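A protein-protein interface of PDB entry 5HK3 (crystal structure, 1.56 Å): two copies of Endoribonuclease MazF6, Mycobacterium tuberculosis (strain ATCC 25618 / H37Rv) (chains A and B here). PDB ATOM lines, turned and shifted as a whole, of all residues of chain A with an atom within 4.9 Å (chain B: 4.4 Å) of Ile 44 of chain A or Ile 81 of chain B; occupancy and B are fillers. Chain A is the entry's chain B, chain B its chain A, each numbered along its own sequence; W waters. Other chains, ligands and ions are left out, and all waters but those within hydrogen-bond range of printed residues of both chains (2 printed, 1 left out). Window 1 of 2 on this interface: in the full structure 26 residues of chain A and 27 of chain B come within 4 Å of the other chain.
The backbone carbonyl oxygen (O) of Ile 81 of chain B is in hydrogen-bond range of the side-chain hydroxyl (OG1) of Thr 83 of chain A.
The backbone carbonyl oxygen of Ile 30 of chain A lies close to the backbone carbonyl oxygen of Leu 112 of chain B.
The backbone NH of Ile 30 of chain B lies within hydrogen-bond range of the backbone carbonyl oxygen of Ile 44 of chain B.
O of Ile 44 of chain A is in hydrogen-bond range of N of Ile 30 of chain A, at 3.0 Å.
The side-chain amide nitrogen (NE2) of Gln 31 of chain A is in hydrogen-bond range of the backbone carbonyl oxygen (O) of Thr 42 of chain A (3.0 Å).
N of Gln 31 of chain A sits at hydrogen-bond distance from O of Ile 44 of chain A, at 3.3 Å.
N of Val 82 of chain A sits at hydrogen-bond distance from O of Ala 45 of chain A.
Among the printed residues, merely in contact across the chains: Gln 31 of chain A with Val 111 of chain B (3.5 Å), Ile 44 of chain A with Val 111 of chain B (3.5 Å), Ile 44 of chain A with Thr 79 of chain B (3.6 Å), Thr 83 of chain A with Thr 79 of chain B (3.6 Å), Ile 81 of chain A with Ile 81 of chain B (3.7 Å), Ile 81 of chain A with Ile 44 of chain B (3.7 Å), Ile 44 of chain A with Ile 81 of chain B (3.7 Å), Thr 83 of chain A with Ala 80 of chain B (3.9 Å) and Val 82 of chain A with Ile 81 of chain B (3.996 Å).
Of the printed residues of chain A, Ile 81 of chain B touches Ile 44 (3.7 Å), Ile 81 (3.7 Å), Val 82 (3.996 Å) and Thr 83 (2.7 Å).
Of the printed residues of chain A, Ile 44 of chain B touches Ile 81 (3.7 Å).
Of the printed residues of chain B, Thr 83 of chain A touches Thr 79 (3.6 Å), Ala 80 (3.9 Å) and Ile 81 (2.7 Å).
Of the printed residues of chain B, Ile 81 of chain A touches Ile 44 and Ile 81.
Of the printed residues of chain B, Val 82 of chain A touches Ile 81 (3.996 Å).
Leu 28 of chain A touches none of the printed residues of chain B.
The nearest residue of chain B that does not touch Ile 44 of chain A is Leu 112 of chain B (4.1 Å).
The nearest printed residue of chain A that does not touch Ile 81 of chain B is Ile 30 of chain A (7.1 Å).
Of the 12 printed residues of chain A, 6 touch a printed residue of chain B.
Hydrophobic or aromatic side chains of chain A within 4 Å of the printed part of chain B: Ile 30, Ile 44 and Ile 81.
Among the printed residues, no Asp or Glu carboxylate lies within 4 Å of a Lys or Arg side-chain nitrogen of the other chain.
Ile 44 of chain A touches Ile 81 of chain B, and with the chains exchanged Ile 81 of chain A touches Ile 44 of chain B.
Ile 81 of chain A touches its own counterpart, Ile 81 of chain B.
Val 82 of chain A touches Ile 81 of chain B, but with the chains exchanged Ile 81 of chain A does not touch Val 82 of chain B (4.03 Å).
6 positions are printed for both chains.
Water W2 lies within hydrogen-bond range of the side-chain hydroxyl of Thr 42 of chain A (2.7 Å), the side-chain amide oxygen of Gln 31 of chain A (2.8 Å), the backbone carbonyl oxygen of Thr 79 of chain B (2.8 Å) and the backbone NH of Val 43 of chain A (3.5 Å).
Water W1 lies within hydrogen-bond range of N of Thr 83 of chain A (2.9 Å) and O of Ile 81 of chain B (3.0 Å).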
ATOM      1  N   LEU A  28      14.515 -15.856   7.645  1.00  0.00           N
ATOM      2  CA  LEU A  28      15.826 -15.330   7.329  1.00  0.00           C
ATOM      3  C   LEU A  28      16.539 -14.929   8.614  1.00  0.00           C
ATOM      4  O   LEU A  28      16.049 -14.067   9.336  1.00  0.00           O
ATOM      5  CB  LEU A  28      15.680 -14.113   6.416  1.00  0.00           C
ATOM      6  CG  LEU A  28      16.972 -13.355   6.133  1.00  0.00           C
ATOM      7  CD1 LEU A  28      17.914 -14.228   5.317  1.00  0.00           C
ATOM      8  CD2 LEU A  28      16.679 -12.037   5.427  1.00  0.00           C
ATOM      9  N   VAL A  29      17.682 -15.540   8.905  1.00  0.00           N
ATOM     10  CA  VAL A  29      18.419 -15.196  10.123  1.00  0.00           C
ATOM     11  C   VAL A  29      18.966 -13.778  10.008  1.00  0.00           C
ATOM     12  O   VAL A  29      19.699 -13.469   9.068  1.00  0.00           O
ATOM     13  CB  VAL A  29      19.565 -16.192  10.385  1.00  0.00           C
ATOM     14  CG1 VAL A  29      20.345 -15.803  11.648  1.00  0.00           C
ATOM     15  CG2 VAL A  29      19.010 -17.601  10.504  1.00  0.00           C
ATOM     16  N   ILE A  30      18.606 -12.913  10.957  1.00  0.00           N
ATOM     17  CA  ILE A  30      19.109 -11.534  10.948  1.00  0.00           C
ATOM     18  C   ILE A  30      19.963 -11.224  12.174  1.00  0.00           C
ATOM     19  O   ILE A  30      20.580 -10.165  12.263  1.00  0.00           O
ATOM     20  CB  ILE A  30      17.958 -10.499  10.842  1.00  0.00           C
ATOM     21  CG1 ILE A  30      16.946 -10.651  11.981  1.00  0.00           C
ATOM     22  CG2 ILE A  30      17.253 -10.640   9.483  1.00  0.00           C
ATOM     23  CD1 ILE A  30      15.892  -9.535  12.020  1.00  0.00           C
ATOM     24  N   GLN A  31      19.998 -12.152  13.118  1.00  0.00           N
ATOM     25  CA  GLN A  31      20.891 -12.047  14.259  1.00  0.00           C
ATOM     26  C   GLN A  31      22.349 -12.144  13.817  1.00  0.00           C
ATOM     27  O   GLN A  31      22.679 -12.910  12.902  1.00  0.00           O
ATOM     28  CB  GLN A  31      20.556 -13.144  15.254  1.00  0.00           C
ATOM     29  CG  GLN A  31      21.404 -13.174  16.508  1.00  0.00           C
ATOM     30  CD  GLN A  31      20.756 -14.039  17.540  1.00  0.00           C
ATOM     31  OE1 GLN A  31      19.770 -13.640  18.147  1.00  0.00           O
ATOM     32  NE2 GLN A  31      21.282 -15.245  17.730  1.00  0.00           N
ATOM     33  N   THR A  42      18.797 -18.844  21.366  1.00  0.00           N
ATOM     34  CA  THR A  42      17.811 -18.362  20.412  1.00  0.00           C
ATOM     35  C   THR A  42      18.441 -17.603  19.261  1.00  0.00           C
ATOM     36  O   THR A  42      19.613 -17.241  19.302  1.00  0.00           O
ATOM     37  CB  THR A  42      16.787 -17.441  21.096  1.00  0.00           C
ATOM     38  OG1 THR A  42      17.477 -16.401  21.803  1.00  0.00           O
ATOM     39  CG2 THR A  42      15.943 -18.230  22.095  1.00  0.00           C
ATOM     40  N   VAL A  43      17.644 -17.407  18.214  1.00  0.00           N
ATOM     41  CA  VAL A  43      18.066 -16.653  17.057  1.00  0.00           C
ATOM     42  C   VAL A  43      16.900 -15.795  16.580  1.00  0.00           C
ATOM     43  O   VAL A  43      15.752 -16.248  16.543  1.00  0.00           O
ATOM     44  CB  VAL A  43      18.554 -17.603  15.939  1.00  0.00           C
ATOM     45  CG1 VAL A  43      17.538 -18.716  15.701  1.00  0.00           C
ATOM     46  CG2 VAL A  43      18.838 -16.855  14.662  1.00  0.00           C
ATOM     47  N   ILE A  44      17.202 -14.563  16.195  1.00  0.00           N
ATOM     48  CA  ILE A  44      16.205 -13.663  15.650  1.00  0.00           C
ATOM     49  C   ILE A  44      16.153 -13.799  14.136  1.00  0.00           C
ATOM     50  O   ILE A  44      17.192 -13.858  13.468  1.00  0.00           O
ATOM     51  CB  ILE A  44      16.515 -12.202  16.022  1.00  0.00           C
ATOM     52  CG1 ILE A  44      16.561 -12.045  17.538  1.00  0.00           C
ATOM     53  CG2 ILE A  44      15.463 -11.274  15.472  1.00  0.00           C
ATOM     54  CD1 ILE A  44      17.265 -10.797  17.960  1.00  0.00           C
ATOM     55  N   ALA A  45      14.938 -13.831  13.601  1.00  0.00           N
ATOM     56  CA  ALA A  45      14.750 -14.013  12.161  1.00  0.00           C
ATOM     57  C   ALA A  45      13.604 -13.169  11.637  1.00  0.00           C
ATOM     58  O   ALA A  45      12.685 -12.832  12.378  1.00  0.00           O
ATOM     59  CB  ALA A  45      14.500 -15.499  11.854  1.00  0.00           C
ATOM     60  N   ALA A  46      13.669 -12.821  10.353  1.00  0.00           N
ATOM     61  CA  ALA A  46      12.555 -12.179   9.671  1.00  0.00           C
ATOM     62  C   ALA A  46      11.774 -13.232   8.902  1.00  0.00           C
ATOM     63  O   ALA A  46      12.352 -14.142   8.314  1.00  0.00           O
ATOM     64  CB  ALA A  46      13.047 -11.088   8.722  1.00  0.00           C
ATOM     65  N   ILE A  81       9.031 -10.121  12.792  1.00  0.00           N
ATOM     66  CA  ILE A  81      10.274 -10.568  13.387  1.00  0.00           C
ATOM     67  C   ILE A  81       9.947 -11.613  14.447  1.00  0.00           C
ATOM     68  O   ILE A  81       9.010 -11.449  15.229  1.00  0.00           O
ATOM     69  CB  ILE A  81      11.056  -9.388  14.006  1.00  0.00           C
ATOM     70  CG1 ILE A  81      11.300  -8.289  12.969  1.00  0.00           C
ATOM     71  CG2 ILE A  81      12.381  -9.869  14.577  1.00  0.00           C
ATOM     72  CD1 ILE A  81      11.997  -8.762  11.729  1.00  0.00           C
ATOM     73  N   VAL A  82      10.700 -12.701  14.459  1.00  0.00           N
ATOM     74  CA  VAL A  82      10.464 -13.748  15.450  1.00  0.00           C
ATOM     75  C   VAL A  82      11.762 -14.131  16.133  1.00  0.00           C
ATOM     76  O   VAL A  82      12.843 -13.978  15.576  1.00  0.00           O
ATOM     77  CB  VAL A  82       9.821 -15.013  14.825  1.00  0.00           C
ATOM     78  CG1 VAL A  82       8.418 -14.703  14.331  1.00  0.00           C
ATOM     79  CG2 VAL A  82      10.688 -15.592  13.698  1.00  0.00           C
ATOM     80  N   THR A  83      11.649 -14.629  17.354  1.00  0.00           N
ATOM     81  CA  THR A  83      12.801 -15.189  18.037  1.00  0.00           C
ATOM     82  C   THR A  83      12.555 -16.676  18.212  1.00  0.00           C
ATOM     83  O   THR A  83      11.544 -17.071  18.789  1.00  0.00           O
ATOM     84  CB  THR A  83      13.036 -14.506  19.391  1.00  0.00           C
ATOM     85  OG1 THR A  83      13.239 -13.107  19.170  1.00  0.00           O
ATOM     86  CG2 THR A  83      14.270 -15.079  20.082  1.00  0.00           C
ATOM     87  N   ILE B  30       9.759  -1.200  19.971  1.00  0.00           N
ATOM     88  CA  ILE B  30      10.954  -0.737  19.269  1.00  0.00           C
ATOM     89  C   ILE B  30      10.670  -0.416  17.800  1.00  0.00           C
ATOM     90  O   ILE B  30      11.518   0.146  17.105  1.00  0.00           O
ATOM     91  CB  ILE B  30      12.115  -1.753  19.379  1.00  0.00           C
ATOM     92  CG1 ILE B  30      11.731  -3.127  18.823  1.00  0.00           C
ATOM     93  CG2 ILE B  30      12.556  -1.876  20.848  1.00  0.00           C
ATOM     94  CD1 ILE B  30      12.916  -4.077  18.744  1.00  0.00           C
ATOM     95  N   ILE B  44       6.570  -4.446  16.634  1.00  0.00           N
ATOM     96  CA  ILE B  44       7.747  -5.169  17.099  1.00  0.00           C
ATOM     97  C   ILE B  44       8.192  -4.625  18.449  1.00  0.00           C
ATOM     98  O   ILE B  44       8.228  -3.411  18.652  1.00  0.00           O
ATOM     99  CB  ILE B  44       8.889  -5.060  16.089  1.00  0.00           C
ATOM    100  CG1 ILE B  44       8.445  -5.645  14.752  1.00  0.00           C
ATOM    101  CG2 ILE B  44      10.110  -5.812  16.559  1.00  0.00           C
ATOM    102  CD1 ILE B  44       9.310  -5.215  13.606  1.00  0.00           C
ATOM    103  N   ALA B  45       8.517  -5.527  19.370  1.00  0.00           N
ATOM    104  CA  ALA B  45       8.888  -5.139  20.726  1.00  0.00           C
ATOM    105  C   ALA B  45       9.993  -6.044  21.274  1.00  0.00           C
ATOM    106  O   ALA B  45      10.157  -7.170  20.819  1.00  0.00           O
ATOM    107  CB  ALA B  45       7.668  -5.181  21.636  1.00  0.00           C
ATOM    108  N   ALA B  46      10.763  -5.529  22.228  1.00  0.00           N
ATOM    109  CA  ALA B  46      11.765  -6.313  22.948  1.00  0.00           C
ATOM    110  C   ALA B  46      11.212  -6.699  24.313  1.00  0.00           C
ATOM    111  O   ALA B  46      10.543  -5.902  24.954  1.00  0.00           O
ATOM    112  CB  ALA B  46      13.061  -5.525  23.093  1.00  0.00           C
ATOM    113  N   VAL B  78      17.682  -7.519  24.644  1.00  0.00           N
ATOM    114  CA  VAL B  78      17.746  -7.114  23.243  1.00  0.00           C
ATOM    115  C   VAL B  78      17.857  -8.281  22.262  1.00  0.00           C
ATOM    116  O   VAL B  78      17.768  -8.050  21.056  1.00  0.00           O
ATOM    117  CB  VAL B  78      18.911  -6.127  22.987  1.00  0.00           C
ATOM    118  CG1 VAL B  78      18.620  -4.772  23.637  1.00  0.00           C
ATOM    119  CG2 VAL B  78      20.222  -6.687  23.492  1.00  0.00           C
ATOM    120  N   THR B  79      18.014  -9.517  22.754  1.00  0.00           N
ATOM    121  CA  THR B  79      17.973 -10.685  21.861  1.00  0.00           C
ATOM    122  C   THR B  79      16.602 -11.369  21.839  1.00  0.00           C
ATOM    123  O   THR B  79      16.405 -12.360  21.129  1.00  0.00           O
ATOM    124  CB  THR B  79      19.037 -11.747  22.242  1.00  0.00           C
ATOM    125  OG1 THR B  79      18.746 -12.289  23.539  1.00  0.00           O
ATOM    126  CG2 THR B  79      20.432 -11.138  22.240  1.00  0.00           C
ATOM    127  N   ALA B  80      15.656 -10.830  22.603  1.00  0.00           N
ATOM    128  CA  ALA B  80      14.307 -11.381  22.695  1.00  0.00           C
ATOM    129  C   ALA B  80      13.316 -10.441  22.037  1.00  0.00           C
ATOM    130  O   ALA B  80      12.770  -9.542  22.675  1.00  0.00           O
ATOM    131  CB  ALA B  80      13.926 -11.620  24.162  1.00  0.00           C
ATOM    132  N   ILE B  81      13.092 -10.658  20.747  1.00  0.00           N
ATOM    133  CA  ILE B  81      12.266  -9.767  19.951  1.00  0.00           C
ATOM    134  C   ILE B  81      10.976 -10.484  19.560  1.00  0.00           C
ATOM    135  O   ILE B  81      10.990 -11.658  19.176  1.00  0.00           O
ATOM    136  CB  ILE B  81      13.015  -9.291  18.698  1.00  0.00           C
ATOM    137  CG1 ILE B  81      14.370  -8.692  19.073  1.00  0.00           C
ATOM    138  CG2 ILE B  81      12.166  -8.308  17.907  1.00  0.00           C
ATOM    139  CD1 ILE B  81      14.291  -7.593  20.100  1.00  0.00           C
ATOM    140  N   VAL B  82       9.857  -9.786  19.695  1.00  0.00           N
ATOM    141  CA  VAL B  82       8.557 -10.347  19.370  1.00  0.00           C
ATOM    142  C   VAL B  82       7.760  -9.406  18.475  1.00  0.00           C
ATOM    143  O   VAL B  82       7.987  -8.199  18.456  1.00  0.00           O
ATOM    144  CB  VAL B  82       7.727 -10.661  20.638  1.00  0.00           C
ATOM    145  CG1 VAL B  82       8.366 -11.785  21.440  1.00  0.00           C
ATOM    146  CG2 VAL B  82       7.558  -9.422  21.500  1.00  0.00           C
ATOM    147  N   LEU B 108      20.470  -3.139  20.144  1.00  0.00           N
ATOM    148  CA  LEU B 108      19.788  -3.731  18.991  1.00  0.00           C
ATOM    149  C   LEU B 108      20.691  -3.734  17.755  1.00  0.00           C
ATOM    150  O   LEU B 108      20.718  -4.713  17.004  1.00  0.00           O
ATOM    151  CB  LEU B 108      18.479  -2.990  18.691  1.00  0.00           C
ATOM    152  CG  LEU B 108      17.360  -3.112  19.737  1.00  0.00           C
ATOM    153  CD1 LEU B 108      16.249  -2.117  19.420  1.00  0.00           C
ATOM    154  CD2 LEU B 108      16.801  -4.523  19.811  1.00  0.00           C
ATOM    155  N   VAL B 111      23.074  -6.604  18.186  1.00  0.00           N
ATOM    156  CA  VAL B 111      22.434  -7.909  18.034  1.00  0.00           C
ATOM    157  C   VAL B 111      22.075  -8.214  16.585  1.00  0.00           C
ATOM    158  O   VAL B 111      22.138  -9.371  16.164  1.00  0.00           O
ATOM    159  CB  VAL B 111      21.167  -7.992  18.903  1.00  0.00           C
ATOM    160  CG1 VAL B 111      20.373  -9.254  18.626  1.00  0.00           C
ATOM    161  CG2 VAL B 111      21.550  -7.938  20.386  1.00  0.00           C
ATOM    162  N   LEU B 112      21.746  -7.183  15.812  1.00  0.00           N
ATOM    163  CA  LEU B 112      21.264  -7.403  14.450  1.00  0.00           C
ATOM    164  C   LEU B 112      22.285  -7.045  13.383  1.00  0.00           C
ATOM    165  O   LEU B 112      21.964  -7.088  12.194  1.00  0.00           O
ATOM    166  CB  LEU B 112      19.986  -6.607  14.202  1.00  0.00           C
ATOM    167  CG  LEU B 112      18.798  -6.922  15.101  1.00  0.00           C
ATOM    168  CD1 LEU B 112      17.684  -5.916  14.867  1.00  0.00           C
ATOM    169  CD2 LEU B 112      18.307  -8.338  14.828  1.00  0.00           C
HETATM  170  O   HOH W   1       9.228 -14.076  18.768  1.00  0.00           O
HETATM  171  O   HOH W   2      17.858 -14.439  19.990  1.00  0.00           O
